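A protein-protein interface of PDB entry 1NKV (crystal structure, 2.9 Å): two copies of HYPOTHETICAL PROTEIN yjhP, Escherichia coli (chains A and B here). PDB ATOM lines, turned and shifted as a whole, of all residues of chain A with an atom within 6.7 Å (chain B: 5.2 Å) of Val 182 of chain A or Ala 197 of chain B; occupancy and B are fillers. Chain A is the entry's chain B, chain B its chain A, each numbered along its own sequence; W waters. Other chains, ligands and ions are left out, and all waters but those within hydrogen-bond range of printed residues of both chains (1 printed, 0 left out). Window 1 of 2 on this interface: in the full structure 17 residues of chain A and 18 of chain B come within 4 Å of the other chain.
NE1 of Trp 200 of chain B lies within hydrogen-bond range of O of Glu 196 of chain B, 3.4 Å away.
The backbone NH of Asp 180 of chain A is in hydrogen-bond range of the backbone carbonyl oxygen of Ile 246 of chain A, at 3.2 Å.
The backbone carbonyl oxygen (O) of Ala 244 of chain A lies within hydrogen-bond range of the backbone NH (N) of Val 182 of chain A, at 3.1 Å.
N of Ala 244 of chain A lies within hydrogen-bond range of O of Glu 183 of chain A (2.9 Å).
The side-chain carboxylate of Glu 183 of chain A is in salt-bridge range of the guanidinium group of Arg 194 of chain B, at 3.3 Å.
O of Met 184 of chain A sits at hydrogen-bond distance from NH2 of Arg 194 of chain B (2.6 Å).
The backbone NH (N) of Ala 198 of chain B is in hydrogen-bond range of the side-chain carboxylate (OE2) of Glu 183 of chain A (3.2 Å).
The backbone NH (N) of Leu 201 of chain B is in hydrogen-bond range of the backbone carbonyl oxygen (O) of Val 182 of chain A, 3.2 Å away.
NH1 of Arg 204 of chain B lies within salt-bridge range of OD2 of Asp 180 of chain A, at 3.0 Å.
The backbone carbonyl oxygen (O) of Val 182 of chain A sits close to the backbone carbonyl oxygen (O) of Ala 197 of chain B, 3.1 Å away.
OE2 of Glu 183 of chain A sits close to O of Ala 197 of chain B (3.2 Å).
Printed residues of chain B within 4 Å of Val 31 of chain A: Arg 194 (3.6 Å) and Leu 201 (3.6 Å).
Of the printed residues of chain B, Asp 180 of chain A touches Arg 204 (3.0 Å).
Phe 243 of chain A touches none of the printed residues of chain B.
Ala 197 of chain B touches just these residues of chain A: Val 182, Glu 183 and Met 184.
Printed residues of chain A within 4 Å of Ala 198 of chain B: Glu 183.
Printed residues of chain A within 4 Å of Trp 200 of chain B: Val 181 (3.2 Å) and Val 182 (3.6 Å).
The nearest printed residue of chain B that does not touch Val 182 of chain A is Arg 204 of chain B (4.02 Å).
The nearest residue of chain A that does not touch Ala 197 of chain B is Val 181 of chain A (5.8 Å).
The nearest printed residue of chain B that does not touch Glu 183 of chain A is Trp 200 of chain B (4.3 Å).
Among the printed residues, pairs that only touch across the chains: Val 31 of chain A with Arg 194 of chain B (3.6 Å), Val 31 of chain A with Leu 201 of chain B (3.6 Å), Val 181 of chain A with Trp 200 of chain B (3.2 Å), Val 182 of chain A with Trp 200 of chain B (3.6 Å), Glu 183 of chain A with Leu 201 of chain B (3.99 Å), Met 184 of chain A with Asp 193 of chain B (3.2 Å), Met 184 of chain A with Ala 197 of chain B (3.9 Å), Val 185 of chain A with Arg 194 of chain B (3.96 Å) and Ile 246 of chain A with Arg 204 of chain B (3.7 Å).
Of the 11 printed residues of chain B, 7 touch a printed residue of chain A.
Printed residues of chain B that touch a printed residue of chain A: Asp 193, Arg 194, Ala 197, Ala 198, Trp 200, Leu 201 and Arg 204.
Among the printed residues, 16 pairs touch across the chains.
Among the printed residues, Asp or Glu carboxylates within 4 Å of a Lys or Arg side-chain nitrogen of the other chain: Asp 180 of chain A with Arg 204 of chain B and Glu 183 of chain A with Arg 194 of chain B.
Water W1 lies within hydrogen-bond range of O of Arg 194 of chain B (2.6 Å), OE2 of Glu 183 of chain A (2.9 Å) and N of Ala 198 of chain B (3.4 Å).
No position is printed for both chains.
Of the 16 pairs that touch across the chains among the printed residues, none has its exchanged pair printed and touching as well.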
ATOM      1  N   VAL A  31      -1.350  26.148  -5.955  1.00  0.00           N
ATOM      2  CA  VAL A  31      -0.296  26.095  -4.958  1.00  0.00           C
ATOM      3  C   VAL A  31       0.901  26.900  -5.449  1.00  0.00           C
ATOM      4  O   VAL A  31       1.699  27.412  -4.666  1.00  0.00           O
ATOM      5  CB  VAL A  31       0.103  24.636  -4.715  1.00  0.00           C
ATOM      6  CG1 VAL A  31       1.360  24.289  -5.513  1.00  0.00           C
ATOM      7  CG2 VAL A  31       0.273  24.388  -3.256  1.00  0.00           C
ATOM      8  N   LEU A  32       1.029  27.009  -6.762  1.00  0.00           N
ATOM      9  CA  LEU A  32       2.140  27.743  -7.327  1.00  0.00           C
ATOM     10  C   LEU A  32       1.859  29.245  -7.269  1.00  0.00           C
ATOM     11  O   LEU A  32       2.680  30.056  -7.690  1.00  0.00           O
ATOM     12  CB  LEU A  32       2.378  27.267  -8.759  1.00  0.00           C
ATOM     13  CG  LEU A  32       3.692  26.532  -9.014  1.00  0.00           C
ATOM     14  CD1 LEU A  32       4.087  25.633  -7.855  1.00  0.00           C
ATOM     15  CD2 LEU A  32       3.526  25.736 -10.292  1.00  0.00           C
ATOM     16  N   ILE A 135      10.254  29.952 -11.705  1.00  0.00           N
ATOM     17  CA  ILE A 135       9.873  28.660 -11.188  1.00  0.00           C
ATOM     18  C   ILE A 135      10.139  27.567 -12.197  1.00  0.00           C
ATOM     19  O   ILE A 135       9.880  27.733 -13.386  1.00  0.00           O
ATOM     20  CB  ILE A 135       8.405  28.611 -10.826  1.00  0.00           C
ATOM     21  CG1 ILE A 135       8.133  29.529  -9.637  1.00  0.00           C
ATOM     22  CG2 ILE A 135       8.008  27.176 -10.532  1.00  0.00           C
ATOM     23  CD1 ILE A 135       6.703  29.531  -9.187  1.00  0.00           C
ATOM     24  N   MET A 136      10.655  26.441 -11.710  1.00  0.00           N
ATOM     25  CA  MET A 136      10.932  25.292 -12.563  1.00  0.00           C
ATOM     26  C   MET A 136      10.236  24.027 -12.064  1.00  0.00           C
ATOM     27  O   MET A 136      10.562  23.515 -10.999  1.00  0.00           O
ATOM     28  CB  MET A 136      12.430  25.035 -12.648  1.00  0.00           C
ATOM     29  CG  MET A 136      12.789  23.822 -13.495  1.00  0.00           C
ATOM     30  SD  MET A 136      14.687  23.663 -13.710  1.00  0.00           S
ATOM     31  CE  MET A 136      15.005  22.099 -12.627  1.00  0.00           C
ATOM     32  N   ASP A 180      16.178  25.395  -4.737  1.00  0.00           N
ATOM     33  CA  ASP A 180      15.534  25.022  -3.502  1.00  0.00           C
ATOM     34  C   ASP A 180      14.093  24.651  -3.855  1.00  0.00           C
ATOM     35  O   ASP A 180      13.479  25.242  -4.744  1.00  0.00           O
ATOM     36  CB  ASP A 180      15.643  26.109  -2.396  1.00  0.00           C
ATOM     37  CG  ASP A 180      15.344  27.504  -2.881  1.00  0.00           C
ATOM     38  OD1 ASP A 180      14.760  27.648  -3.968  1.00  0.00           O
ATOM     39  OD2 ASP A 180      15.673  28.464  -2.158  1.00  0.00           O
ATOM     40  N   VAL A 181      13.602  23.595  -3.214  1.00  0.00           N
ATOM     41  CA  VAL A 181      12.262  23.107  -3.459  1.00  0.00           C
ATOM     42  C   VAL A 181      11.295  24.100  -2.824  1.00  0.00           C
ATOM     43  O   VAL A 181      11.272  24.267  -1.605  1.00  0.00           O
ATOM     44  CB  VAL A 181      12.115  21.687  -2.859  1.00  0.00           C
ATOM     45  CG1 VAL A 181      10.750  21.084  -3.191  1.00  0.00           C
ATOM     46  CG2 VAL A 181      13.231  20.812  -3.404  1.00  0.00           C
ATOM     47  N   VAL A 182      10.517  24.801  -3.636  1.00  0.00           N
ATOM     48  CA  VAL A 182       9.605  25.774  -3.062  1.00  0.00           C
ATOM     49  C   VAL A 182       8.195  25.237  -3.013  1.00  0.00           C
ATOM     50  O   VAL A 182       7.350  25.749  -2.294  1.00  0.00           O
ATOM     51  CB  VAL A 182       9.646  27.111  -3.840  1.00  0.00           C
ATOM     52  CG1 VAL A 182      10.981  27.761  -3.613  1.00  0.00           C
ATOM     53  CG2 VAL A 182       9.400  26.890  -5.322  1.00  0.00           C
ATOM     54  N   GLU A 183       7.946  24.184  -3.772  1.00  0.00           N
ATOM     55  CA  GLU A 183       6.635  23.570  -3.787  1.00  0.00           C
ATOM     56  C   GLU A 183       6.788  22.173  -4.335  1.00  0.00           C
ATOM     57  O   GLU A 183       7.710  21.877  -5.101  1.00  0.00           O
ATOM     58  CB  GLU A 183       5.670  24.376  -4.644  1.00  0.00           C
ATOM     59  CG  GLU A 183       4.650  25.212  -3.876  1.00  0.00           C
ATOM     60  CD  GLU A 183       3.820  24.404  -2.873  1.00  0.00           C
ATOM     61  OE1 GLU A 183       3.445  23.257  -3.171  1.00  0.00           O
ATOM     62  OE2 GLU A 183       3.523  24.924  -1.784  1.00  0.00           O
ATOM     63  N   MET A 184       5.877  21.305  -3.939  1.00  0.00           N
ATOM     64  CA  MET A 184       5.950  19.925  -4.378  1.00  0.00           C
ATOM     65  C   MET A 184       4.615  19.219  -4.242  1.00  0.00           C
ATOM     66  O   MET A 184       4.046  19.157  -3.149  1.00  0.00           O
ATOM     67  CB  MET A 184       7.013  19.203  -3.548  1.00  0.00           C
ATOM     68  CG  MET A 184       6.765  17.726  -3.325  1.00  0.00           C
ATOM     69  SD  MET A 184       8.035  17.021  -2.084  1.00  0.00           S
ATOM     70  CE  MET A 184       6.961  16.789  -0.508  1.00  0.00           C
ATOM     71  N   VAL A 185       4.134  18.677  -5.358  1.00  0.00           N
ATOM     72  CA  VAL A 185       2.879  17.936  -5.380  1.00  0.00           C
ATOM     73  C   VAL A 185       3.114  16.526  -5.869  1.00  0.00           C
ATOM     74  O   VAL A 185       3.326  16.310  -7.057  1.00  0.00           O
ATOM     75  CB  VAL A 185       1.862  18.578  -6.293  1.00  0.00           C
ATOM     76  CG1 VAL A 185       0.690  17.637  -6.451  1.00  0.00           C
ATOM     77  CG2 VAL A 185       1.410  19.911  -5.709  1.00  0.00           C
ATOM     78  N   PHE A 243       8.057  18.690  -8.905  1.00  0.00           N
ATOM     79  CA  PHE A 243       8.730  19.534  -7.929  1.00  0.00           C
ATOM     80  C   PHE A 243       8.997  20.913  -8.524  1.00  0.00           C
ATOM     81  O   PHE A 243       9.613  21.026  -9.582  1.00  0.00           O
ATOM     82  CB  PHE A 243      10.074  18.942  -7.509  1.00  0.00           C
ATOM     83  CG  PHE A 243       9.996  17.546  -6.984  1.00  0.00           C
ATOM     84  CD1 PHE A 243       9.912  16.469  -7.851  1.00  0.00           C
ATOM     85  CD2 PHE A 243      10.032  17.306  -5.618  1.00  0.00           C
ATOM     86  CE1 PHE A 243       9.866  15.171  -7.368  1.00  0.00           C
ATOM     87  CE2 PHE A 243       9.986  16.016  -5.122  1.00  0.00           C
ATOM     88  CZ  PHE A 243       9.903  14.945  -6.000  1.00  0.00           C
ATOM     89  N   ALA A 244       8.535  21.955  -7.837  1.00  0.00           N
ATOM     90  CA  ALA A 244       8.743  23.322  -8.283  1.00  0.00           C
ATOM     91  C   ALA A 244      10.057  23.738  -7.663  1.00  0.00           C
ATOM     92  O   ALA A 244      10.273  23.558  -6.468  1.00  0.00           O
ATOM     93  CB  ALA A 244       7.633  24.209  -7.811  1.00  0.00           C
ATOM     94  N   LEU A 245      10.936  24.305  -8.479  1.00  0.00           N
ATOM     95  CA  LEU A 245      12.251  24.699  -8.012  1.00  0.00           C
ATOM     96  C   LEU A 245      12.647  26.086  -8.460  1.00  0.00           C
ATOM     97  O   LEU A 245      12.406  26.453  -9.607  1.00  0.00           O
ATOM     98  CB  LEU A 245      13.277  23.728  -8.564  1.00  0.00           C
ATOM     99  CG  LEU A 245      12.920  22.260  -8.547  1.00  0.00           C
ATOM    100  CD1 LEU A 245      14.061  21.517  -9.167  1.00  0.00           C
ATOM    101  CD2 LEU A 245      12.655  21.771  -7.122  1.00  0.00           C
ATOM    102  N   ILE A 246      13.274  26.845  -7.569  1.00  0.00           N
ATOM    103  CA  ILE A 246      13.755  28.175  -7.926  1.00  0.00           C
ATOM    104  C   ILE A 246      15.255  28.233  -7.648  1.00  0.00           C
ATOM    105  O   ILE A 246      15.691  27.921  -6.555  1.00  0.00           O
ATOM    106  CB  ILE A 246      13.049  29.292  -7.127  1.00  0.00           C
ATOM    107  CG1 ILE A 246      11.570  29.369  -7.518  1.00  0.00           C
ATOM    108  CG2 ILE A 246      13.722  30.634  -7.419  1.00  0.00           C
ATOM    109  CD1 ILE A 246      10.816  30.510  -6.866  1.00  0.00           C
ATOM    110  N   TRP B 192      -0.131  16.901   4.681  1.00  0.00           N
ATOM    111  CA  TRP B 192       1.110  17.355   5.243  1.00  0.00           C
ATOM    112  C   TRP B 192       1.855  18.098   4.151  1.00  0.00           C
ATOM    113  O   TRP B 192       2.313  19.205   4.378  1.00  0.00           O
ATOM    114  CB  TRP B 192       1.956  16.186   5.743  1.00  0.00           C
ATOM    115  CG  TRP B 192       1.760  15.865   7.184  1.00  0.00           C
ATOM    116  CD1 TRP B 192       0.916  14.936   7.710  1.00  0.00           C
ATOM    117  CD2 TRP B 192       2.406  16.491   8.295  1.00  0.00           C
ATOM    118  NE1 TRP B 192       0.994  14.940   9.084  1.00  0.00           N
ATOM    119  CE2 TRP B 192       1.903  15.888   9.469  1.00  0.00           C
ATOM    120  CE3 TRP B 192       3.363  17.507   8.413  1.00  0.00           C
ATOM    121  CZ2 TRP B 192       2.324  16.268  10.752  1.00  0.00           C
ATOM    122  CZ3 TRP B 192       3.781  17.886   9.692  1.00  0.00           C
ATOM    123  CH2 TRP B 192       3.258  17.264  10.841  1.00  0.00           C
ATOM    124  N   ASP B 193       1.954  17.536   2.951  1.00  0.00           N
ATOM    125  CA  ASP B 193       2.703  18.244   1.917  1.00  0.00           C
ATOM    126  C   ASP B 193       2.237  19.668   1.680  1.00  0.00           C
ATOM    127  O   ASP B 193       3.043  20.593   1.624  1.00  0.00           O
ATOM    128  CB  ASP B 193       2.654  17.516   0.584  1.00  0.00           C
ATOM    129  CG  ASP B 193       3.351  16.207   0.626  1.00  0.00           C
ATOM    130  OD1 ASP B 193       4.409  16.114   1.283  1.00  0.00           O
ATOM    131  OD2 ASP B 193       2.847  15.259  -0.010  1.00  0.00           O
ATOM    132  N   ARG B 194       0.933  19.839   1.516  1.00  0.00           N
ATOM    133  CA  ARG B 194       0.379  21.153   1.265  1.00  0.00           C
ATOM    134  C   ARG B 194       0.771  22.118   2.388  1.00  0.00           C
ATOM    135  O   ARG B 194       0.965  23.308   2.154  1.00  0.00           O
ATOM    136  CB  ARG B 194      -1.147  21.053   1.133  1.00  0.00           C
ATOM    137  CG  ARG B 194      -1.646  20.236  -0.069  1.00  0.00           C
ATOM    138  CD  ARG B 194      -1.381  20.946  -1.400  1.00  0.00           C
ATOM    139  NE  ARG B 194       0.049  21.173  -1.608  1.00  0.00           N
ATOM    140  CZ  ARG B 194       0.945  20.200  -1.768  1.00  0.00           C
ATOM    141  NH1 ARG B 194       0.565  18.928  -1.765  1.00  0.00           N
ATOM    142  NH2 ARG B 194       2.225  20.501  -1.881  1.00  0.00           N
ATOM    143  N   TYR B 195       0.914  21.585   3.598  1.00  0.00           N
ATOM    144  CA  TYR B 195       1.271  22.379   4.757  1.00  0.00           C
ATOM    145  C   TYR B 195       2.751  22.786   4.782  1.00  0.00           C
ATOM    146  O   TYR B 195       3.070  23.970   4.931  1.00  0.00           O
ATOM    147  CB  TYR B 195       0.881  21.612   6.029  1.00  0.00           C
ATOM    148  CG  TYR B 195       1.237  22.307   7.318  1.00  0.00           C
ATOM    149  CD1 TYR B 195       0.821  23.611   7.565  1.00  0.00           C
ATOM    150  CD2 TYR B 195       2.043  21.680   8.265  1.00  0.00           C
ATOM    151  CE1 TYR B 195       1.208  24.277   8.712  1.00  0.00           C
ATOM    152  CE2 TYR B 195       2.437  22.336   9.416  1.00  0.00           C
ATOM    153  CZ  TYR B 195       2.023  23.632   9.632  1.00  0.00           C
ATOM    154  OH  TYR B 195       2.453  24.300  10.758  1.00  0.00           O
ATOM    155  N   GLU B 196       3.650  21.813   4.632  1.00  0.00           N
ATOM    156  CA  GLU B 196       5.089  22.072   4.626  1.00  0.00           C
ATOM    157  C   GLU B 196       5.531  22.787   3.337  1.00  0.00           C
ATOM    158  O   GLU B 196       6.217  23.812   3.394  1.00  0.00           O
ATOM    159  CB  GLU B 196       5.857  20.769   4.780  1.00  0.00           C
ATOM    160  CG  GLU B 196       5.682  20.122   6.131  1.00  0.00           C
ATOM    161  CD  GLU B 196       6.165  20.997   7.285  1.00  0.00           C
ATOM    162  OE1 GLU B 196       7.007  21.907   7.029  1.00  0.00           O
ATOM    163  OE2 GLU B 196       5.718  20.763   8.444  1.00  0.00           O
ATOM    164  N   ALA B 197       5.136  22.254   2.181  1.00  0.00           N
ATOM    165  CA  ALA B 197       5.494  22.879   0.918  1.00  0.00           C
ATOM    166  C   ALA B 197       5.107  24.359   0.894  1.00  0.00           C
ATOM    167  O   ALA B 197       5.873  25.192   0.430  1.00  0.00           O
ATOM    168  CB  ALA B 197       4.836  22.160  -0.241  1.00  0.00           C
ATOM    169  N   ALA B 198       3.933  24.714   1.398  1.00  0.00           N
ATOM    170  CA  ALA B 198       3.569  26.123   1.367  1.00  0.00           C
ATOM    171  C   ALA B 198       4.671  26.981   2.013  1.00  0.00           C
ATOM    172  O   ALA B 198       5.139  27.950   1.407  1.00  0.00           O
ATOM    173  CB  ALA B 198       2.208  26.362   2.046  1.00  0.00           C
ATOM    174  N   LYS B 199       5.099  26.620   3.219  1.00  0.00           N
ATOM    175  CA  LYS B 199       6.144  27.371   3.903  1.00  0.00           C
ATOM    176  C   LYS B 199       7.381  27.597   3.034  1.00  0.00           C
ATOM    177  O   LYS B 199       7.976  28.676   3.061  1.00  0.00           O
ATOM    178  CB  LYS B 199       6.584  26.647   5.175  1.00  0.00           C
ATOM    179  CG  LYS B 199       5.455  26.201   6.073  1.00  0.00           C
ATOM    180  CD  LYS B 199       6.029  25.397   7.219  1.00  0.00           C
ATOM    181  CE  LYS B 199       4.969  24.817   8.117  1.00  0.00           C
ATOM    182  NZ  LYS B 199       5.663  24.172   9.250  1.00  0.00           N
ATOM    183  N   TRP B 200       7.776  26.586   2.266  1.00  0.00           N
ATOM    184  CA  TRP B 200       8.962  26.741   1.434  1.00  0.00           C
ATOM    185  C   TRP B 200       8.807  27.846   0.391  1.00  0.00           C
ATOM    186  O   TRP B 200       9.782  28.484   0.019  1.00  0.00           O
ATOM    187  CB  TRP B 200       9.338  25.436   0.726  1.00  0.00           C
ATOM    188  CG  TRP B 200       9.369  24.234   1.597  1.00  0.00           C
ATOM    189  CD1 TRP B 200       9.533  24.200   2.941  1.00  0.00           C
ATOM    190  CD2 TRP B 200       9.190  22.879   1.176  1.00  0.00           C
ATOM    191  NE1 TRP B 200       9.458  22.902   3.394  1.00  0.00           N
ATOM    192  CE2 TRP B 200       9.245  22.073   2.327  1.00  0.00           C
ATOM    193  CE3 TRP B 200       8.985  22.268  -0.069  1.00  0.00           C
ATOM    194  CZ2 TRP B 200       9.101  20.687   2.280  1.00  0.00           C
ATOM    195  CZ3 TRP B 200       8.845  20.886  -0.116  1.00  0.00           C
ATOM    196  CH2 TRP B 200       8.903  20.112   1.059  1.00  0.00           C
ATOM    197  N   LEU B 201       7.590  28.086  -0.075  1.00  0.00           N
ATOM    198  CA  LEU B 201       7.381  29.105  -1.085  1.00  0.00           C
ATOM    199  C   LEU B 201       7.145  30.447  -0.453  1.00  0.00           C
ATOM    200  O   LEU B 201       7.468  31.477  -1.028  1.00  0.00           O
ATOM    201  CB  LEU B 201       6.179  28.759  -1.947  1.00  0.00           C
ATOM    202  CG  LEU B 201       5.942  29.699  -3.122  1.00  0.00           C
ATOM    203  CD1 LEU B 201       7.191  29.774  -3.984  1.00  0.00           C
ATOM    204  CD2 LEU B 201       4.755  29.202  -3.932  1.00  0.00           C
ATOM    205  N   ARG B 204      10.608  31.785   0.721  1.00  0.00           N
ATOM    206  CA  ARG B 204      11.375  32.228  -0.426  1.00  0.00           C
ATOM    207  C   ARG B 204      10.786  33.552  -0.923  1.00  0.00           C
ATOM    208  O   ARG B 204      11.524  34.488  -1.223  1.00  0.00           O
ATOM    209  CB  ARG B 204      11.322  31.191  -1.550  1.00  0.00           C
ATOM    210  CG  ARG B 204      11.994  31.654  -2.836  1.00  0.00           C
ATOM    211  CD  ARG B 204      13.493  31.734  -2.655  1.00  0.00           C
ATOM    212  NE  ARG B 204      14.182  32.473  -3.725  1.00  0.00           N
ATOM    213  CZ  ARG B 204      15.263  32.026  -4.365  1.00  0.00           C
ATOM    214  NH1 ARG B 204      15.783  30.841  -4.062  1.00  0.00           N
ATOM    215  NH2 ARG B 204      15.828  32.775  -5.293  1.00  0.00           N
HETATM  216  O   HOH W   1       1.198  23.860  -0.421  1.00  0.00           O
